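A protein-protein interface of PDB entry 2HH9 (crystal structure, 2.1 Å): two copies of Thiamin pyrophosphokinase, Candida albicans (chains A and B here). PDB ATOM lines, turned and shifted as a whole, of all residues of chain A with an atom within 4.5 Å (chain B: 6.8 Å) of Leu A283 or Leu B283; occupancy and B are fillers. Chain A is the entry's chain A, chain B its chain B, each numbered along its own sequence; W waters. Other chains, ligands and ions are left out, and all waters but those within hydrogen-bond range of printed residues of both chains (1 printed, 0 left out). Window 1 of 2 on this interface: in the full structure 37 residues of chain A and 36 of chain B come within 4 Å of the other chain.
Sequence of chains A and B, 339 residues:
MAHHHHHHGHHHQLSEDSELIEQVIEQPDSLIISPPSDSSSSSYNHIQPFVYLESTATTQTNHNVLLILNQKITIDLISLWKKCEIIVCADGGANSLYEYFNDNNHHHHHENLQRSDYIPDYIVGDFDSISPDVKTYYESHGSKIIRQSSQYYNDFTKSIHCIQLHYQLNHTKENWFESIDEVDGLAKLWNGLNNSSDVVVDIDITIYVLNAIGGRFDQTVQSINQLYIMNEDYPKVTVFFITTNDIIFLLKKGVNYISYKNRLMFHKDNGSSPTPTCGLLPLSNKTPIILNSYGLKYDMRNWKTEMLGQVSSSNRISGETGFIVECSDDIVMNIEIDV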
ATOM      1  N   PHE A 217      28.173 -31.779 -24.826  1.00  0.00           N
ATOM      2  CA  PHE A 217      28.486 -30.765 -23.832  1.00  0.00           C
ATOM      3  C   PHE A 217      28.327 -31.168 -22.363  1.00  0.00           C
ATOM      4  O   PHE A 217      29.121 -30.754 -21.524  1.00  0.00           O
ATOM      5  CB  PHE A 217      27.665 -29.497 -24.108  1.00  0.00           C
ATOM      6  CG  PHE A 217      28.190 -28.273 -23.409  1.00  0.00           C
ATOM      7  CD1 PHE A 217      29.487 -27.829 -23.644  1.00  0.00           C
ATOM      8  CD2 PHE A 217      27.390 -27.559 -22.526  1.00  0.00           C
ATOM      9  CE1 PHE A 217      29.982 -26.689 -23.011  1.00  0.00           C
ATOM     10  CE2 PHE A 217      27.877 -26.414 -21.886  1.00  0.00           C
ATOM     11  CZ  PHE A 217      29.173 -25.982 -22.132  1.00  0.00           C
ATOM     12  N   VAL A 221      31.231 -30.876 -19.511  1.00  0.00           N
ATOM     13  CA  VAL A 221      31.058 -30.236 -18.218  1.00  0.00           C
ATOM     14  C   VAL A 221      31.284 -31.184 -17.039  1.00  0.00           C
ATOM     15  O   VAL A 221      31.898 -30.800 -16.044  1.00  0.00           O
ATOM     16  CB  VAL A 221      29.669 -29.580 -18.106  1.00  0.00           C
ATOM     17  CG1 VAL A 221      29.478 -29.000 -16.710  1.00  0.00           C
ATOM     18  CG2 VAL A 221      29.544 -28.467 -19.155  1.00  0.00           C
ATOM     19  N   ILE A 224      34.916 -31.545 -16.496  1.00  0.00           N
ATOM     20  CA  ILE A 224      35.501 -30.382 -15.840  1.00  0.00           C
ATOM     21  C   ILE A 224      35.132 -30.402 -14.348  1.00  0.00           C
ATOM     22  O   ILE A 224      35.961 -30.101 -13.491  1.00  0.00           O
ATOM     23  CB  ILE A 224      35.014 -29.068 -16.508  1.00  0.00           C
ATOM     24  CG1 ILE A 224      35.586 -28.965 -17.932  1.00  0.00           C
ATOM     25  CG2 ILE A 224      35.449 -27.862 -15.684  1.00  0.00           C
ATOM     26  CD1 ILE A 224      37.122 -28.932 -18.006  1.00  0.00           C
ATOM     27  N   TYR A 228      37.832 -30.516 -10.988  1.00  0.00           N
ATOM     28  CA  TYR A 228      37.830 -29.710  -9.770  1.00  0.00           C
ATOM     29  C   TYR A 228      37.694 -30.578  -8.520  1.00  0.00           C
ATOM     30  O   TYR A 228      38.432 -30.406  -7.554  1.00  0.00           O
ATOM     31  CB  TYR A 228      36.667 -28.714  -9.788  1.00  0.00           C
ATOM     32  CG  TYR A 228      36.908 -27.446 -10.572  1.00  0.00           C
ATOM     33  CD1 TYR A 228      37.650 -26.395 -10.031  1.00  0.00           C
ATOM     34  CD2 TYR A 228      36.353 -27.276 -11.843  1.00  0.00           C
ATOM     35  CE1 TYR A 228      37.827 -25.202 -10.731  1.00  0.00           C
ATOM     36  CE2 TYR A 228      36.522 -26.088 -12.553  1.00  0.00           C
ATOM     37  CZ  TYR A 228      37.255 -25.056 -11.991  1.00  0.00           C
ATOM     38  OH  TYR A 228      37.391 -23.872 -12.676  1.00  0.00           O
ATOM     39  N   LEU A 281      39.605 -20.132 -17.293  1.00  0.00           N
ATOM     40  CA  LEU A 281      38.160 -20.287 -17.174  1.00  0.00           C
ATOM     41  C   LEU A 281      37.651 -20.598 -15.767  1.00  0.00           C
ATOM     42  O   LEU A 281      37.855 -21.695 -15.243  1.00  0.00           O
ATOM     43  CB  LEU A 281      37.733 -21.371 -18.173  1.00  0.00           C
ATOM     44  CG  LEU A 281      38.608 -21.265 -19.438  1.00  0.00           C
ATOM     45  CD1 LEU A 281      38.476 -22.504 -20.298  1.00  0.00           C
ATOM     46  CD2 LEU A 281      38.239 -20.012 -20.219  1.00  0.00           C
ATOM     47  N   PRO A 282      36.960 -19.627 -15.147  1.00  0.00           N
ATOM     48  CA  PRO A 282      36.401 -19.740 -13.795  1.00  0.00           C
ATOM     49  C   PRO A 282      35.129 -20.593 -13.772  1.00  0.00           C
ATOM     50  O   PRO A 282      34.019 -20.065 -13.682  1.00  0.00           O
ATOM     51  CB  PRO A 282      36.149 -18.284 -13.421  1.00  0.00           C
ATOM     52  CG  PRO A 282      35.678 -17.699 -14.721  1.00  0.00           C
ATOM     53  CD  PRO A 282      36.595 -18.336 -15.764  1.00  0.00           C
ATOM     54  N   LEU A 283      35.301 -21.912 -13.822  1.00  0.00           N
ATOM     55  CA  LEU A 283      34.167 -22.827 -13.864  1.00  0.00           C
ATOM     56  C   LEU A 283      33.791 -23.565 -12.574  1.00  0.00           C
ATOM     57  O   LEU A 283      33.157 -24.619 -12.630  1.00  0.00           O
ATOM     58  CB  LEU A 283      34.388 -23.845 -14.991  1.00  0.00           C
ATOM     59  CG  LEU A 283      34.550 -23.275 -16.409  1.00  0.00           C
ATOM     60  CD1 LEU A 283      35.175 -24.317 -17.325  1.00  0.00           C
ATOM     61  CD2 LEU A 283      33.198 -22.816 -16.947  1.00  0.00           C
ATOM     62  N   SER A 284      34.169 -23.034 -11.416  1.00  0.00           N
ATOM     63  CA  SER A 284      33.813 -23.689 -10.158  1.00  0.00           C
ATOM     64  C   SER A 284      32.771 -22.850  -9.415  1.00  0.00           C
ATOM     65  O   SER A 284      32.333 -21.814  -9.913  1.00  0.00           O
ATOM     66  CB  SER A 284      35.044 -23.876  -9.270  1.00  0.00           C
ATOM     67  OG  SER A 284      35.452 -22.642  -8.717  1.00  0.00           O
ATOM     68  N   MET A 307      32.080 -16.305 -14.190  1.00  0.00           N
ATOM     69  CA  MET A 307      31.110 -16.504 -15.254  1.00  0.00           C
ATOM     70  C   MET A 307      30.051 -15.448 -14.946  1.00  0.00           C
ATOM     71  O   MET A 307      29.770 -15.185 -13.780  1.00  0.00           O
ATOM     72  CB  MET A 307      30.534 -17.923 -15.186  1.00  0.00           C
ATOM     73  CG  MET A 307      31.555 -18.993 -15.559  1.00  0.00           C
ATOM     74  SD  MET A 307      32.227 -18.756 -17.245  1.00  0.00           S
ATOM     75  CE  MET A 307      30.885 -19.521 -18.228  1.00  0.00           C
ATOM     76  N   PHE B 217      38.636 -24.704 -26.204  1.00  0.00           N
ATOM     77  CA  PHE B 217      37.873 -24.631 -24.969  1.00  0.00           C
ATOM     78  C   PHE B 217      37.571 -23.239 -24.418  1.00  0.00           C
ATOM     79  O   PHE B 217      36.484 -23.016 -23.895  1.00  0.00           O
ATOM     80  CB  PHE B 217      38.540 -25.476 -23.875  1.00  0.00           C
ATOM     81  CG  PHE B 217      37.622 -25.797 -22.729  1.00  0.00           C
ATOM     82  CD1 PHE B 217      36.403 -26.423 -22.960  1.00  0.00           C
ATOM     83  CD2 PHE B 217      37.966 -25.469 -21.425  1.00  0.00           C
ATOM     84  CE1 PHE B 217      35.536 -26.718 -21.908  1.00  0.00           C
ATOM     85  CE2 PHE B 217      37.106 -25.760 -20.364  1.00  0.00           C
ATOM     86  CZ  PHE B 217      35.892 -26.385 -20.608  1.00  0.00           C
ATOM     87  N   VAL B 221      33.816 -21.644 -23.538  1.00  0.00           N
ATOM     88  CA  VAL B 221      33.427 -21.035 -22.284  1.00  0.00           C
ATOM     89  C   VAL B 221      32.990 -19.582 -22.455  1.00  0.00           C
ATOM     90  O   VAL B 221      32.021 -19.150 -21.837  1.00  0.00           O
ATOM     91  CB  VAL B 221      34.562 -21.130 -21.255  1.00  0.00           C
ATOM     92  CG1 VAL B 221      34.178 -20.378 -19.983  1.00  0.00           C
ATOM     93  CG2 VAL B 221      34.841 -22.606 -20.941  1.00  0.00           C
ATOM     94  N   ILE B 224      29.476 -19.610 -23.584  1.00  0.00           N
ATOM     95  CA  ILE B 224      28.520 -19.900 -22.522  1.00  0.00           C
ATOM     96  C   ILE B 224      28.399 -18.691 -21.588  1.00  0.00           C
ATOM     97  O   ILE B 224      27.316 -18.384 -21.098  1.00  0.00           O
ATOM     98  CB  ILE B 224      28.942 -21.149 -21.713  1.00  0.00           C
ATOM     99  CG1 ILE B 224      28.852 -22.400 -22.600  1.00  0.00           C
ATOM    100  CG2 ILE B 224      28.046 -21.312 -20.488  1.00  0.00           C
ATOM    101  CD1 ILE B 224      27.440 -22.699 -23.131  1.00  0.00           C
ATOM    102  N   ASN B 225      29.516 -18.012 -21.344  1.00  0.00           N
ATOM    103  CA  ASN B 225      29.525 -16.832 -20.480  1.00  0.00           C
ATOM    104  C   ASN B 225      28.585 -15.788 -21.090  1.00  0.00           C
ATOM    105  O   ASN B 225      27.698 -15.264 -20.417  1.00  0.00           O
ATOM    106  CB  ASN B 225      30.957 -16.287 -20.369  1.00  0.00           C
ATOM    107  CG  ASN B 225      31.064 -15.087 -19.440  1.00  0.00           C
ATOM    108  OD1 ASN B 225      30.368 -15.005 -18.431  1.00  0.00           O
ATOM    109  ND2 ASN B 225      31.962 -14.160 -19.769  1.00  0.00           N
ATOM    110  N   TYR B 228      24.859 -16.457 -20.684  1.00  0.00           N
ATOM    111  CA  TYR B 228      24.328 -16.029 -19.390  1.00  0.00           C
ATOM    112  C   TYR B 228      24.144 -14.509 -19.336  1.00  0.00           C
ATOM    113  O   TYR B 228      23.086 -14.009 -18.953  1.00  0.00           O
ATOM    114  CB  TYR B 228      25.271 -16.459 -18.261  1.00  0.00           C
ATOM    115  CG  TYR B 228      25.084 -17.883 -17.772  1.00  0.00           C
ATOM    116  CD1 TYR B 228      23.990 -18.234 -16.975  1.00  0.00           C
ATOM    117  CD2 TYR B 228      26.012 -18.877 -18.088  1.00  0.00           C
ATOM    118  CE1 TYR B 228      23.828 -19.546 -16.502  1.00  0.00           C
ATOM    119  CE2 TYR B 228      25.861 -20.192 -17.620  1.00  0.00           C
ATOM    120  CZ  TYR B 228      24.768 -20.518 -16.827  1.00  0.00           C
ATOM    121  OH  TYR B 228      24.619 -21.810 -16.359  1.00  0.00           O
ATOM    122  N   LEU B 281      23.537 -27.968 -16.785  1.00  0.00           N
ATOM    123  CA  LEU B 281      24.865 -27.511 -16.383  1.00  0.00           C
ATOM    124  C   LEU B 281      24.912 -26.166 -15.669  1.00  0.00           C
ATOM    125  O   LEU B 281      24.673 -25.119 -16.269  1.00  0.00           O
ATOM    126  CB  LEU B 281      25.739 -27.504 -17.643  1.00  0.00           C
ATOM    127  CG  LEU B 281      25.346 -28.730 -18.491  1.00  0.00           C
ATOM    128  CD1 LEU B 281      25.842 -28.603 -19.920  1.00  0.00           C
ATOM    129  CD2 LEU B 281      25.869 -29.997 -17.822  1.00  0.00           C
ATOM    130  N   PRO B 282      25.238 -26.185 -14.365  1.00  0.00           N
ATOM    131  CA  PRO B 282      25.321 -24.984 -13.525  1.00  0.00           C
ATOM    132  C   PRO B 282      26.645 -24.252 -13.731  1.00  0.00           C
ATOM    133  O   PRO B 282      27.550 -24.345 -12.902  1.00  0.00           O
ATOM    134  CB  PRO B 282      25.172 -25.555 -12.118  1.00  0.00           C
ATOM    135  CG  PRO B 282      25.961 -26.838 -12.207  1.00  0.00           C
ATOM    136  CD  PRO B 282      25.616 -27.393 -13.603  1.00  0.00           C
ATOM    137  N   LEU B 283      26.744 -23.504 -14.825  1.00  0.00           N
ATOM    138  CA  LEU B 283      27.981 -22.805 -15.152  1.00  0.00           C
ATOM    139  C   LEU B 283      28.028 -21.297 -14.873  1.00  0.00           C
ATOM    140  O   LEU B 283      28.845 -20.585 -15.459  1.00  0.00           O
ATOM    141  CB  LEU B 283      28.331 -23.064 -16.622  1.00  0.00           C
ATOM    142  CG  LEU B 283      28.582 -24.520 -17.041  1.00  0.00           C
ATOM    143  CD1 LEU B 283      28.570 -24.621 -18.559  1.00  0.00           C
ATOM    144  CD2 LEU B 283      29.915 -25.014 -16.476  1.00  0.00           C
ATOM    145  N   SER B 284      27.169 -20.799 -13.992  1.00  0.00           N
ATOM    146  CA  SER B 284      27.189 -19.367 -13.684  1.00  0.00           C
ATOM    147  C   SER B 284      27.759 -19.145 -12.284  1.00  0.00           C
ATOM    148  O   SER B 284      28.105 -20.104 -11.591  1.00  0.00           O
ATOM    149  CB  SER B 284      25.781 -18.774 -13.761  1.00  0.00           C
ATOM    150  OG  SER B 284      25.027 -19.139 -12.623  1.00  0.00           O
ATOM    151  N   ASN B 285      27.850 -17.882 -11.874  1.00  0.00           N
ATOM    152  CA  ASN B 285      28.382 -17.533 -10.558  1.00  0.00           C
ATOM    153  C   ASN B 285      27.299 -17.574  -9.479  1.00  0.00           C
ATOM    154  O   ASN B 285      27.536 -17.190  -8.335  1.00  0.00           O
ATOM    155  CB  ASN B 285      29.036 -16.142 -10.606  1.00  0.00           C
ATOM    156  CG  ASN B 285      28.028 -15.023 -10.820  1.00  0.00           C
ATOM    157  OD1 ASN B 285      26.973 -15.223 -11.425  1.00  0.00           O
ATOM    158  ND2 ASN B 285      28.359 -13.830 -10.335  1.00  0.00           N
ATOM    159  N   LYS B 286      26.107 -18.032  -9.853  1.00  0.00           N
ATOM    160  CA  LYS B 286      24.998 -18.149  -8.910  1.00  0.00           C
ATOM    161  C   LYS B 286      24.902 -19.627  -8.579  1.00  0.00           C
ATOM    162  O   LYS B 286      24.487 -20.435  -9.410  1.00  0.00           O
ATOM    163  CB  LYS B 286      23.690 -17.661  -9.541  1.00  0.00           C
ATOM    164  CG  LYS B 286      23.686 -16.186  -9.903  1.00  0.00           C
ATOM    165  CD  LYS B 286      22.390 -15.779 -10.590  1.00  0.00           C
ATOM    166  CE  LYS B 286      22.430 -14.318 -11.014  1.00  0.00           C
ATOM    167  NZ  LYS B 286      21.246 -13.927 -11.831  1.00  0.00           N
ATOM    168  N   ILE B 289      22.126 -24.278  -7.573  1.00  0.00           N
ATOM    169  CA  ILE B 289      20.867 -24.145  -8.296  1.00  0.00           C
ATOM    170  C   ILE B 289      19.985 -25.301  -7.835  1.00  0.00           C
ATOM    171  O   ILE B 289      20.423 -26.450  -7.850  1.00  0.00           O
ATOM    172  CB  ILE B 289      21.063 -24.321  -9.823  1.00  0.00           C
ATOM    173  CG1 ILE B 289      22.198 -23.427 -10.330  1.00  0.00           C
ATOM    174  CG2 ILE B 289      19.751 -24.041 -10.549  1.00  0.00           C
ATOM    175  CD1 ILE B 289      21.770 -22.051 -10.758  1.00  0.00           C
ATOM    176  N   MET B 307      28.870 -26.745  -9.664  1.00  0.00           N
ATOM    177  CA  MET B 307      30.160 -27.277 -10.067  1.00  0.00           C
ATOM    178  C   MET B 307      30.864 -27.560  -8.736  1.00  0.00           C
ATOM    179  O   MET B 307      30.654 -26.841  -7.759  1.00  0.00           O
ATOM    180  CB  MET B 307      30.923 -26.254 -10.913  1.00  0.00           C
ATOM    181  CG  MET B 307      30.323 -26.072 -12.308  1.00  0.00           C
ATOM    182  SD  MET B 307      30.207 -27.648 -13.243  1.00  0.00           S
ATOM    183  CE  MET B 307      31.818 -27.662 -14.060  1.00  0.00           C
ATOM    184  N   LEU B 308      31.679 -28.612  -8.702  1.00  0.00           N
ATOM    185  CA  LEU B 308      32.366 -29.047  -7.480  1.00  0.00           C
ATOM    186  C   LEU B 308      31.347 -29.764  -6.598  1.00  0.00           C
ATOM    187  O   LEU B 308      31.573 -29.992  -5.409  1.00  0.00           O
ATOM    188  CB  LEU B 308      32.981 -27.869  -6.712  1.00  0.00           C
ATOM    189  CG  LEU B 308      34.457 -27.565  -6.990  1.00  0.00           C
ATOM    190  CD1 LEU B 308      34.904 -26.371  -6.162  1.00  0.00           C
ATOM    191  CD2 LEU B 308      35.304 -28.782  -6.638  1.00  0.00           C
ATOM    192  N   ASP B 330      18.977 -19.154 -13.504  1.00  0.00           N
ATOM    193  CA  ASP B 330      19.263 -19.552 -14.878  1.00  0.00           C
ATOM    194  C   ASP B 330      20.276 -20.683 -14.884  1.00  0.00           C
ATOM    195  O   ASP B 330      21.222 -20.685 -14.092  1.00  0.00           O
ATOM    196  CB  ASP B 330      19.850 -18.393 -15.686  1.00  0.00           C
ATOM    197  CG  ASP B 330      18.891 -17.232 -15.845  1.00  0.00           C
ATOM    198  OD1 ASP B 330      17.692 -17.371 -15.525  1.00  0.00           O
ATOM    199  OD2 ASP B 330      19.353 -16.172 -16.312  1.00  0.00           O
ATOM    200  N   ILE B 331      20.073 -21.647 -15.775  1.00  0.00           N
ATOM    201  CA  ILE B 331      20.997 -22.763 -15.885  1.00  0.00           C
ATOM    202  C   ILE B 331      21.022 -23.281 -17.318  1.00  0.00           C
ATOM    203  O   ILE B 331      20.006 -23.260 -18.019  1.00  0.00           O
ATOM    204  CB  ILE B 331      20.624 -23.896 -14.902  1.00  0.00           C
ATOM    205  CG1 ILE B 331      21.655 -25.026 -15.007  1.00  0.00           C
ATOM    206  CG2 ILE B 331      19.194 -24.400 -15.185  1.00  0.00           C
ATOM    207  CD1 ILE B 331      21.581 -26.034 -13.876  1.00  0.00           C
ATOM    208  N   VAL B 332      22.196 -23.714 -17.759  1.00  0.00           N
ATOM    209  CA  VAL B 332      22.367 -24.226 -19.110  1.00  0.00           C
ATOM    210  C   VAL B 332      21.824 -25.643 -19.266  1.00  0.00           C
ATOM    211  O   VAL B 332      21.943 -26.462 -18.360  1.00  0.00           O
ATOM    212  CB  VAL B 332      23.858 -24.269 -19.509  1.00  0.00           C
ATOM    213  CG1 VAL B 332      24.021 -25.012 -20.827  1.00  0.00           C
ATOM    214  CG2 VAL B 332      24.424 -22.850 -19.604  1.00  0.00           C
HETATM  215  O   HOH W   1      30.632 -19.841 -10.275  1.00  0.00           O
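The backbone carbonyl oxygen (O) of Leu A281 is in hydrogen-bond range of the side-chain hydroxyl (OH) of Tyr A228, at 3.4 Å.
The side-chain hydroxyl of Tyr A228 is in hydrogen-bond range of the backbone NH of Leu A283.
OH of Tyr B228 is in hydrogen-bond range of O of Leu B281 (3.3 Å).
The side-chain hydroxyl (OH) of Tyr B228 sits at hydrogen-bond distance from the backbone NH (N) of Leu B283 (3.1 Å).
N of Leu B281 sits at hydrogen-bond distance from O of Val B332 (2.7 Å).
OG of Ser B284 sits close to N of Lys B286, 3.2 Å away.
Phe A217 touches Ile B224.
CD2 of Phe A217 touches CD1 of Leu B281, at 3.2 Å.
Leu B283 touches Phe A217 (CD1 to CE2, 3.8 Å).
Phe B217 touches Ile A224.
Met B307 touches Ile A224 (CE to CG2, 3.98 Å).
Phe B217 touches Leu A283 (CE2 to CD1, 3.9 Å).
CB of Met B307 touches CA of Ser A284 (3.9 Å).
Leu B308 touches Ser A284 (CD1 to CB, 3.99 Å).
Met A307 touches Val B221 (SD to CG1, 3.7 Å).
C of Met A307 touches OD1 of Asn B225 (3.5 Å).
Printed residues of chain B within 4 Å of Tyr A228: Leu B308 (3.4 Å).
Printed residues of chain B within 4 Å of Leu A283: Phe B217 (3.9 Å), Leu B283 (3.98 Å) and Met B307 (3.2 Å).
Of the printed residues of chain A, Val B221 touches Leu A281 and Met A307.
Printed residues of chain A within 4 Å of Ile B224: Phe A217.
Printed residues of chain A within 4 Å of Asn B225: Met A307.
Printed residues of chain A within 4 Å of Met B307: Val A221 (3.7 Å), Ile A224 (3.98 Å), Leu A283 (3.2 Å) and Ser A284 (3.9 Å).
Asp B330 touches none of the printed residues of chain A.
The nearest printed residue of chain B that does not touch Leu A283 is Val B221 (4.01 Å).
The nearest printed residue of chain A that does not touch Leu B283 is Val A221 (4.01 Å).
The nearest printed residue of chain A that does not touch Asn B285 is Ser A284 (5.9 Å).
Of the 17 printed residues of chain B, 10 touch a printed residue of chain A.
Hydrophobic or aromatic side chains of chain B that line the printed part of chain A: Phe B217, Val B221, Ile B224, Leu B281, Leu B283, Met B307 and Leu B308.
Hydrophobic or aromatic side chains of chain A that line the printed part of chain B: Phe A217, Val A221, Ile A224, Tyr A228, Leu A281, Leu A283 and Met A307.
Among the printed residues, 20 pairs touch across the chains.
Among the printed residues, no Asp or Glu carboxylate lies within 4 Å of a Lys or Arg side-chain nitrogen of the other chain.
Phe A217 touches Ile B224, and with the chains exchanged Ile A224 touches Phe B217.
Phe A217 touches Leu B281, and with the chains exchanged Leu A281 touches Phe B217.
Phe A217 touches Leu B283, and with the chains exchanged Leu A283 touches Phe B217.
Leu B283 touches its own counterpart, Leu A283.
Of the 20 pairs that touch across the chains among the printed residues, 15 have their exchanged pair printed and touching as well.
Water W1 bridges the backbone carbonyl oxygen of Ser A284 and the backbone carbonyl oxygen of Ser B284.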
